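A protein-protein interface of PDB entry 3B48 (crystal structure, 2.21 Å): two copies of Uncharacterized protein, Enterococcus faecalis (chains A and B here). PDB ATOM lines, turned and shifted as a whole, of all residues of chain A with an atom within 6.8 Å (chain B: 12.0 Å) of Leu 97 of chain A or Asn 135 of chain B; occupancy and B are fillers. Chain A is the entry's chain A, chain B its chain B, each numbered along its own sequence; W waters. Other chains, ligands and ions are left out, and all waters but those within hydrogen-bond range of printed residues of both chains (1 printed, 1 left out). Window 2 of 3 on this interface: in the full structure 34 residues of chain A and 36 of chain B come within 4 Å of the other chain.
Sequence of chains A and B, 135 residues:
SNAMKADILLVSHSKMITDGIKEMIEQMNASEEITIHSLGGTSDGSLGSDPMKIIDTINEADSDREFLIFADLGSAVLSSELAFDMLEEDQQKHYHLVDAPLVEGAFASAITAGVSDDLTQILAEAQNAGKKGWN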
ATOM      1  N   PHE A  67      -3.387 -26.677   4.413  1.00  0.00           N
ATOM      2  CA  PHE A  67      -4.438 -26.478   3.422  1.00  0.00           C
ATOM      3  C   PHE A  67      -4.821 -25.036   3.418  1.00  0.00           C
ATOM      4  O   PHE A  67      -5.277 -24.485   4.421  1.00  0.00           O
ATOM      5  CB  PHE A  67      -5.676 -27.332   3.733  1.00  0.00           C
ATOM      6  CG  PHE A  67      -5.348 -28.761   3.999  1.00  0.00           C
ATOM      7  CD1 PHE A  67      -5.025 -29.621   2.944  1.00  0.00           C
ATOM      8  CD2 PHE A  67      -5.284 -29.239   5.302  1.00  0.00           C
ATOM      9  CE1 PHE A  67      -4.676 -30.950   3.195  1.00  0.00           C
ATOM     10  CE2 PHE A  67      -4.921 -30.569   5.558  1.00  0.00           C
ATOM     11  CZ  PHE A  67      -4.633 -31.419   4.495  1.00  0.00           C
ATOM     12  N   LEU A  68      -4.607 -24.402   2.273  1.00  0.00           N
ATOM     13  CA  LEU A  68      -4.895 -22.996   2.145  1.00  0.00           C
ATOM     14  C   LEU A  68      -6.147 -22.949   1.321  1.00  0.00           C
ATOM     15  O   LEU A  68      -6.124 -23.340   0.178  1.00  0.00           O
ATOM     16  CB  LEU A  68      -3.732 -22.257   1.473  1.00  0.00           C
ATOM     17  CG  LEU A  68      -2.362 -22.517   2.080  1.00  0.00           C
ATOM     18  CD1 LEU A  68      -1.296 -21.696   1.389  1.00  0.00           C
ATOM     19  CD2 LEU A  68      -2.356 -22.236   3.550  1.00  0.00           C
ATOM     20  N   ILE A  69      -7.239 -22.495   1.916  1.00  0.00           N
ATOM     21  CA  ILE A  69      -8.517 -22.394   1.187  1.00  0.00           C
ATOM     22  C   ILE A  69      -8.728 -21.008   0.584  1.00  0.00           C
ATOM     23  O   ILE A  69      -8.675 -20.003   1.308  1.00  0.00           O
ATOM     24  CB  ILE A  69      -9.764 -22.844   2.036  1.00  0.00           C
ATOM     25  CG1 ILE A  69      -9.789 -24.372   2.212  1.00  0.00           C
ATOM     26  CG2 ILE A  69     -11.083 -22.395   1.353  1.00  0.00           C
ATOM     27  CD1 ILE A  69      -8.693 -24.962   3.098  1.00  0.00           C
ATOM     28  N   PHE A  70      -8.954 -20.967  -0.731  1.00  0.00           N
ATOM     29  CA  PHE A  70      -9.314 -19.721  -1.423  1.00  0.00           C
ATOM     30  C   PHE A  70     -10.699 -19.854  -2.020  1.00  0.00           C
ATOM     31  O   PHE A  70     -10.990 -20.860  -2.635  1.00  0.00           O
ATOM     32  CB  PHE A  70      -8.297 -19.401  -2.525  1.00  0.00           C
ATOM     33  CG  PHE A  70      -6.913 -19.149  -2.009  1.00  0.00           C
ATOM     34  CD1 PHE A  70      -6.512 -17.857  -1.652  1.00  0.00           C
ATOM     35  CD2 PHE A  70      -6.014 -20.208  -1.847  1.00  0.00           C
ATOM     36  CE1 PHE A  70      -5.223 -17.629  -1.182  1.00  0.00           C
ATOM     37  CE2 PHE A  70      -4.719 -19.990  -1.357  1.00  0.00           C
ATOM     38  CZ  PHE A  70      -4.328 -18.710  -1.031  1.00  0.00           C
ATOM     39  N   VAL A  77     -17.592 -19.084   0.084  1.00  0.00           N
ATOM     40  CA  VAL A  77     -17.151 -18.720   1.428  1.00  0.00           C
ATOM     41  C   VAL A  77     -17.920 -19.474   2.543  1.00  0.00           C
ATOM     42  O   VAL A  77     -17.319 -20.039   3.466  1.00  0.00           O
ATOM     43  CB  VAL A  77     -17.238 -17.155   1.627  1.00  0.00           C
ATOM     44  CG1 VAL A  77     -17.119 -16.764   3.077  1.00  0.00           C
ATOM     45  CG2 VAL A  77     -16.144 -16.431   0.813  1.00  0.00           C
ATOM     46  N   SER A  80     -16.899 -23.239   2.403  1.00  0.00           N
ATOM     47  CA  SER A  80     -15.548 -23.428   2.938  1.00  0.00           C
ATOM     48  C   SER A  80     -15.528 -23.374   4.447  1.00  0.00           C
ATOM     49  O   SER A  80     -14.663 -23.984   5.079  1.00  0.00           O
ATOM     50  CB  SER A  80     -14.620 -22.301   2.442  1.00  0.00           C
ATOM     51  OG  SER A  80     -14.781 -22.092   1.053  1.00  0.00           O
ATOM     52  N   GLU A  81     -16.427 -22.562   4.998  1.00  0.00           N
ATOM     53  CA  GLU A  81     -16.557 -22.396   6.439  1.00  0.00           C
ATOM     54  C   GLU A  81     -17.254 -23.644   7.029  1.00  0.00           C
ATOM     55  O   GLU A  81     -16.774 -24.226   7.995  1.00  0.00           O
ATOM     56  CB  GLU A  81     -17.304 -21.087   6.778  1.00  0.00           C
ATOM     57  CG  GLU A  81     -16.521 -19.813   6.491  1.00  0.00           C
ATOM     58  CD  GLU A  81     -17.349 -18.522   6.696  1.00  0.00           C
ATOM     59  OE1 GLU A  81     -18.563 -18.511   6.402  1.00  0.00           O
ATOM     60  OE2 GLU A  81     -16.782 -17.501   7.139  1.00  0.00           O
ATOM     61  N   PHE A  84     -14.740 -26.596   7.138  1.00  0.00           N
ATOM     62  CA  PHE A  84     -13.924 -26.467   8.366  1.00  0.00           C
ATOM     63  C   PHE A  84     -14.666 -26.968   9.635  1.00  0.00           C
ATOM     64  O   PHE A  84     -14.137 -27.760  10.427  1.00  0.00           O
ATOM     65  CB  PHE A  84     -13.467 -24.989   8.534  1.00  0.00           C
ATOM     66  CG  PHE A  84     -12.722 -24.701   9.829  1.00  0.00           C
ATOM     67  CD1 PHE A  84     -11.362 -24.970   9.946  1.00  0.00           C
ATOM     68  CD2 PHE A  84     -13.382 -24.130  10.923  1.00  0.00           C
ATOM     69  CE1 PHE A  84     -10.675 -24.684  11.126  1.00  0.00           C
ATOM     70  CE2 PHE A  84     -12.706 -23.859  12.107  1.00  0.00           C
ATOM     71  CZ  PHE A  84     -11.342 -24.135  12.204  1.00  0.00           C
ATOM     72  N   TYR A  95      -5.957 -26.312   8.385  1.00  0.00           N
ATOM     73  CA  TYR A  95      -6.918 -25.811   7.447  1.00  0.00           C
ATOM     74  C   TYR A  95      -6.920 -24.301   7.638  1.00  0.00           C
ATOM     75  O   TYR A  95      -7.232 -23.800   8.714  1.00  0.00           O
ATOM     76  CB  TYR A  95      -8.291 -26.437   7.777  1.00  0.00           C
ATOM     77  CG  TYR A  95      -9.453 -26.151   6.806  1.00  0.00           C
ATOM     78  CD1 TYR A  95      -9.922 -27.146   5.941  1.00  0.00           C
ATOM     79  CD2 TYR A  95     -10.083 -24.898   6.766  1.00  0.00           C
ATOM     80  CE1 TYR A  95     -11.013 -26.912   5.066  1.00  0.00           C
ATOM     81  CE2 TYR A  95     -11.148 -24.641   5.884  1.00  0.00           C
ATOM     82  CZ  TYR A  95     -11.616 -25.654   5.050  1.00  0.00           C
ATOM     83  OH  TYR A  95     -12.662 -25.427   4.194  1.00  0.00           O
ATOM     84  N   HIS A  96      -6.542 -23.585   6.584  1.00  0.00           N
ATOM     85  CA  HIS A  96      -6.448 -22.147   6.638  1.00  0.00           C
ATOM     86  C   HIS A  96      -7.349 -21.495   5.606  1.00  0.00           C
ATOM     87  O   HIS A  96      -7.131 -21.600   4.390  1.00  0.00           O
ATOM     88  CB  HIS A  96      -4.989 -21.718   6.480  1.00  0.00           C
ATOM     89  CG  HIS A  96      -4.062 -22.456   7.393  1.00  0.00           C
ATOM     90  ND1 HIS A  96      -3.846 -22.072   8.704  1.00  0.00           N
ATOM     91  CD2 HIS A  96      -3.341 -23.591   7.214  1.00  0.00           C
ATOM     92  CE1 HIS A  96      -3.001 -22.913   9.281  1.00  0.00           C
ATOM     93  NE2 HIS A  96      -2.690 -23.852   8.404  1.00  0.00           N
ATOM     94  N   LEU A  97      -8.384 -20.838   6.108  1.00  0.00           N
ATOM     95  CA  LEU A  97      -9.230 -19.960   5.305  1.00  0.00           C
ATOM     96  C   LEU A  97      -8.434 -18.689   5.032  1.00  0.00           C
ATOM     97  O   LEU A  97      -8.127 -17.936   5.940  1.00  0.00           O
ATOM     98  CB  LEU A  97     -10.517 -19.641   6.068  1.00  0.00           C
ATOM     99  CG  LEU A  97     -11.460 -20.816   6.370  1.00  0.00           C
ATOM    100  CD1 LEU A  97     -12.584 -20.455   7.400  1.00  0.00           C
ATOM    101  CD2 LEU A  97     -12.064 -21.323   5.094  1.00  0.00           C
ATOM    102  N   VAL A  98      -8.089 -18.457   3.768  1.00  0.00           N
ATOM    103  CA  VAL A  98      -7.196 -17.366   3.478  1.00  0.00           C
ATOM    104  C   VAL A  98      -8.004 -16.168   3.065  1.00  0.00           C
ATOM    105  O   VAL A  98      -8.840 -16.242   2.135  1.00  0.00           O
ATOM    106  CB  VAL A  98      -6.121 -17.696   2.408  1.00  0.00           C
ATOM    107  CG1 VAL A  98      -5.024 -16.586   2.411  1.00  0.00           C
ATOM    108  CG2 VAL A  98      -5.471 -19.084   2.656  1.00  0.00           C
ATOM    109  N   ASP A  99      -7.754 -15.062   3.772  1.00  0.00           N
ATOM    110  CA  ASP A  99      -8.513 -13.832   3.532  1.00  0.00           C
ATOM    111  C   ASP A  99      -7.873 -13.120   2.359  1.00  0.00           C
ATOM    112  O   ASP A  99      -7.134 -12.186   2.549  1.00  0.00           O
ATOM    113  CB  ASP A  99      -8.547 -12.944   4.777  1.00  0.00           C
ATOM    114  CG  ASP A  99      -9.848 -12.142   4.889  1.00  0.00           C
ATOM    115  OD1 ASP A  99     -10.900 -12.644   4.386  1.00  0.00           O
ATOM    116  OD2 ASP A  99      -9.794 -11.008   5.474  1.00  0.00           O
ATOM    117  N   ALA A 100      -8.125 -13.621   1.153  1.00  0.00           N
ATOM    118  CA  ALA A 100      -7.455 -13.126  -0.051  1.00  0.00           C
ATOM    119  C   ALA A 100      -8.403 -13.180  -1.238  1.00  0.00           C
ATOM    120  O   ALA A 100      -9.418 -13.858  -1.151  1.00  0.00           O
ATOM    121  CB  ALA A 100      -6.217 -13.936  -0.334  1.00  0.00           C
ATOM    122  N   LEU A 123       0.632 -16.589   3.735  1.00  0.00           N
ATOM    123  CA  LEU A 123      -0.727 -16.085   3.897  1.00  0.00           C
ATOM    124  C   LEU A 123      -0.738 -14.574   3.826  1.00  0.00           C
ATOM    125  O   LEU A 123      -1.679 -13.981   3.301  1.00  0.00           O
ATOM    126  CB  LEU A 123      -1.325 -16.561   5.231  1.00  0.00           C
ATOM    127  CG  LEU A 123      -1.124 -18.041   5.548  1.00  0.00           C
ATOM    128  CD1 LEU A 123      -1.620 -18.404   6.935  1.00  0.00           C
ATOM    129  CD2 LEU A 123      -1.800 -18.914   4.473  1.00  0.00           C
ATOM    130  N   GLN A 127      -2.872 -12.432   1.489  1.00  0.00           N
ATOM    131  CA  GLN A 127      -3.757 -11.383   2.022  1.00  0.00           C
ATOM    132  C   GLN A 127      -3.573  -9.984   1.411  1.00  0.00           C
ATOM    133  O   GLN A 127      -4.549  -9.224   1.299  1.00  0.00           O
ATOM    134  CB  GLN A 127      -3.659 -11.282   3.560  1.00  0.00           C
ATOM    135  CG  GLN A 127      -4.282 -12.470   4.316  1.00  0.00           C
ATOM    136  CD  GLN A 127      -3.845 -12.553   5.775  1.00  0.00           C
ATOM    137  OE1 GLN A 127      -3.837 -13.630   6.361  1.00  0.00           O
ATOM    138  NE2 GLN A 127      -3.467 -11.421   6.360  1.00  0.00           N
ATOM    139  N   GLU B 104     -13.808 -10.918  -7.621  1.00  0.00           N
ATOM    140  CA  GLU B 104     -14.564 -10.206  -6.621  1.00  0.00           C
ATOM    141  C   GLU B 104     -14.836  -8.749  -6.959  1.00  0.00           C
ATOM    142  O   GLU B 104     -15.932  -8.279  -6.735  1.00  0.00           O
ATOM    143  CB  GLU B 104     -13.929 -10.352  -5.237  1.00  0.00           C
ATOM    144  CG  GLU B 104     -13.771 -11.824  -4.770  1.00  0.00           C
ATOM    145  CD  GLU B 104     -12.409 -12.442  -5.161  1.00  0.00           C
ATOM    146  OE1 GLU B 104     -11.718 -11.946  -6.088  1.00  0.00           O
ATOM    147  OE2 GLU B 104     -12.021 -13.424  -4.523  1.00  0.00           O
ATOM    148  N   GLY B 130     -11.988  -7.894  -2.279  1.00  0.00           N
ATOM    149  CA  GLY B 130     -11.284  -9.177  -2.050  1.00  0.00           C
ATOM    150  C   GLY B 130     -11.425 -10.003  -0.754  1.00  0.00           C
ATOM    151  O   GLY B 130     -11.076 -11.184  -0.736  1.00  0.00           O
ATOM    152  N   LYS B 131     -11.916  -9.411   0.335  1.00  0.00           N
ATOM    153  CA  LYS B 131     -11.867 -10.117   1.624  1.00  0.00           C
ATOM    154  C   LYS B 131     -13.171 -10.824   1.986  1.00  0.00           C
ATOM    155  O   LYS B 131     -14.239 -10.579   1.406  1.00  0.00           O
ATOM    156  CB  LYS B 131     -11.397  -9.208   2.762  1.00  0.00           C
ATOM    157  CG  LYS B 131     -10.275  -8.277   2.372  1.00  0.00           C
ATOM    158  CD  LYS B 131      -8.933  -8.791   2.806  1.00  0.00           C
ATOM    159  CE  LYS B 131      -7.959  -7.634   2.882  1.00  0.00           C
ATOM    160  NZ  LYS B 131      -6.560  -8.112   2.923  1.00  0.00           N
ATOM    161  N   LYS B 132     -13.062 -11.703   2.969  1.00  0.00           N
ATOM    162  CA  LYS B 132     -14.065 -12.737   3.208  1.00  0.00           C
ATOM    163  C   LYS B 132     -14.468 -12.782   4.681  1.00  0.00           C
ATOM    164  O   LYS B 132     -15.394 -13.513   5.035  1.00  0.00           O
ATOM    165  CB  LYS B 132     -13.507 -14.118   2.797  1.00  0.00           C
ATOM    166  CG  LYS B 132     -12.539 -14.165   1.561  1.00  0.00           C
ATOM    167  CD  LYS B 132     -13.292 -14.075   0.294  1.00  0.00           C
ATOM    168  CE  LYS B 132     -12.443 -13.579  -0.839  1.00  0.00           C
ATOM    169  NZ  LYS B 132     -13.328 -12.859  -1.744  1.00  0.00           N
ATOM    170  N   GLY B 133     -13.785 -12.002   5.526  1.00  0.00           N
ATOM    171  CA  GLY B 133     -13.923 -12.102   6.983  1.00  0.00           C
ATOM    172  C   GLY B 133     -13.134 -13.284   7.524  1.00  0.00           C
ATOM    173  O   GLY B 133     -13.588 -13.975   8.454  1.00  0.00           O
ATOM    174  N   TRP B 134     -11.958 -13.528   6.936  1.00  0.00           N
ATOM    175  CA  TRP B 134     -11.144 -14.728   7.223  1.00  0.00           C
ATOM    176  C   TRP B 134      -9.796 -14.456   7.915  1.00  0.00           C
ATOM    177  O   TRP B 134      -9.510 -13.325   8.296  1.00  0.00           O
ATOM    178  CB  TRP B 134     -10.945 -15.560   5.947  1.00  0.00           C
ATOM    179  CG  TRP B 134     -12.150 -16.362   5.572  1.00  0.00           C
ATOM    180  CD1 TRP B 134     -13.324 -16.478   6.283  1.00  0.00           C
ATOM    181  CD2 TRP B 134     -12.300 -17.195   4.418  1.00  0.00           C
ATOM    182  NE1 TRP B 134     -14.201 -17.302   5.619  1.00  0.00           N
ATOM    183  CE2 TRP B 134     -13.598 -17.768   4.480  1.00  0.00           C
ATOM    184  CE3 TRP B 134     -11.468 -17.515   3.332  1.00  0.00           C
ATOM    185  CZ2 TRP B 134     -14.078 -18.677   3.497  1.00  0.00           C
ATOM    186  CZ3 TRP B 134     -11.962 -18.400   2.340  1.00  0.00           C
ATOM    187  CH2 TRP B 134     -13.250 -18.967   2.439  1.00  0.00           C
ATOM    188  N   ASN B 135      -9.000 -15.518   8.069  1.00  0.00           N
ATOM    189  CA  ASN B 135      -7.709 -15.535   8.770  1.00  0.00           C
ATOM    190  C   ASN B 135      -6.958 -16.834   8.444  1.00  0.00           C
ATOM    191  O   ASN B 135      -5.757 -16.839   8.136  1.00  0.00           O
ATOM    192  CB  ASN B 135      -7.889 -15.400  10.325  1.00  0.00           C
ATOM    193  OXT ASN B 135      -7.566 -17.918   8.492  1.00  0.00           O
HETATM  194  O   HOH W   1      -6.794  -8.950   0.134  1.00  0.00           O
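The backbone carbonyl oxygen (O) of Gly 130 of chain B sits close to the backbone carbonyl oxygen (O) of Ala 100 of chain A (3.2 Å).
The backbone carbonyl oxygen of Gln 127 of chain A sits at hydrogen-bond distance from the side-chain amino group of Lys 131 of chain B, 2.8 Å away.
The backbone NH (N) of Gly 133 of chain B is in hydrogen-bond range of the side-chain carboxylate (OD1) of Asp 99 of chain A (3.2 Å).
The side-chain carboxylate of Asp 99 of chain A sits at hydrogen-bond distance from the backbone NH of Lys 132 of chain B, at 2.8 Å.
OD1 of Asp 99 of chain A sits at hydrogen-bond distance from N of Trp 134 of chain B (2.9 Å).
The side-chain carboxylate of Glu 81 of chain A is in hydrogen-bond range of the indole nitrogen of Trp 134 of chain B.
N of Asn 135 of chain B sits close to O of Leu 97 of chain A, at 3.3 Å.
O of Gly 130 of chain B lies close to NZ of Lys 132 of chain B (3.0 Å).
N of Ile 69 of chain A is in hydrogen-bond range of O of His 96 of chain A (2.6 Å).
OE2 of Glu 104 of chain B lies within salt-bridge range of NZ of Lys 132 of chain B.
The backbone carbonyl oxygen (O) of Ser 80 of chain A sits at hydrogen-bond distance from the side-chain hydroxyl (OH) of Tyr 95 of chain A (2.6 Å).
The backbone carbonyl oxygen (O) of Ile 69 of chain A lies within hydrogen-bond range of the backbone NH (N) of Val 98 of chain A.
Ile 69 of chain A touches Trp 134 of chain B.
Val 77 of chain A touches Lys 132 of chain B (CG2 to CD, 3.7 Å).
CZ2 of Trp 134 of chain B touches O of Val 77 of chain A, at 3.5 Å.
CH2 of Trp 134 of chain B touches CB of Ser 80 of chain A, at 3.6 Å.
Trp 134 of chain B touches Leu 97 of chain A.
O of Val 98 of chain A touches CE3 of Trp 134 of chain B (3.2 Å).
Lys 131 of chain B touches Asp 99 of chain A.
CE of Lys 132 of chain B touches O of Ala 100 of chain A, at 3.1 Å.
Of chain B, only Trp 134 (3.4 Å) and Asn 135 (2.6 Å) come within 4 Å of Leu 97 of chain A.
Of chain A, only Leu 97 comes within 4 Å of Asn 135 of chain B.
No residue of chain B comes within 4 Å of Phe 70 of chain A.
Ser 80 of chain A touches one residue of chain B.
Of chain B, only Trp 134 (3.0 Å) comes within 4 Å of Glu 81 of chain A.
Tyr 95 of chain A touches none of the printed residues of chain B.
No residue of chain B comes within 4 Å of His 96 of chain A.
Of chain B, only Trp 134 (3.2 Å) comes within 4 Å of Val 98 of chain A.
Asp 99 of chain A touches just these residues of chain B: Lys 131, Lys 132, Gly 133 and Trp 134.
No residue of chain B comes within 4 Å of Leu 123 of chain A.
Printed residues of chain B within 4 Å of Ala 100 of chain A: Gly 130 (3.2 Å) and Lys 132 (3.1 Å).
Printed residues of chain B within 4 Å of Gln 127 of chain A: Lys 131 (2.8 Å).
Of the printed residues of chain A, Trp 134 of chain B touches Ile 69 (3.8 Å), Val 77 (3.5 Å), Ser 80 (3.6 Å), Glu 81 (3.0 Å), Leu 97 (3.4 Å), Val 98 (3.2 Å) and Asp 99 (2.9 Å).
Of the printed residues of chain A, Lys 132 of chain B touches Val 77 (3.7 Å), Asp 99 (2.8 Å) and Ala 100 (3.1 Å).
Printed residues of chain A within 4 Å of Lys 131 of chain B: Asp 99 (3.6 Å) and Gln 127 (2.8 Å).
The nearest residue of chain A that does not touch Asn 135 of chain B is Gln 127 of chain A (4.1 Å).
Of the 16 printed residues of chain A, 9 touch a printed residue of chain B.
Hydrophobic or aromatic side chains of chain A within 4 Å of the printed part of chain B: Val 77 and Leu 97.
Of the 7 printed residues of chain B, 6 touch a printed residue of chain A.
Among the printed residues, no Asp or Glu carboxylate lies within 4 Å of a Lys or Arg side-chain nitrogen of the other chain.
No position is printed for both chains.
Of the 15 pairs that touch across the chains among the printed residues, none has its exchanged pair printed and touching as well.
Water W1 bridges O of Gln 127 of chain A (2.5 Å) and NZ of Lys 131 of chain B (2.9 Å).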
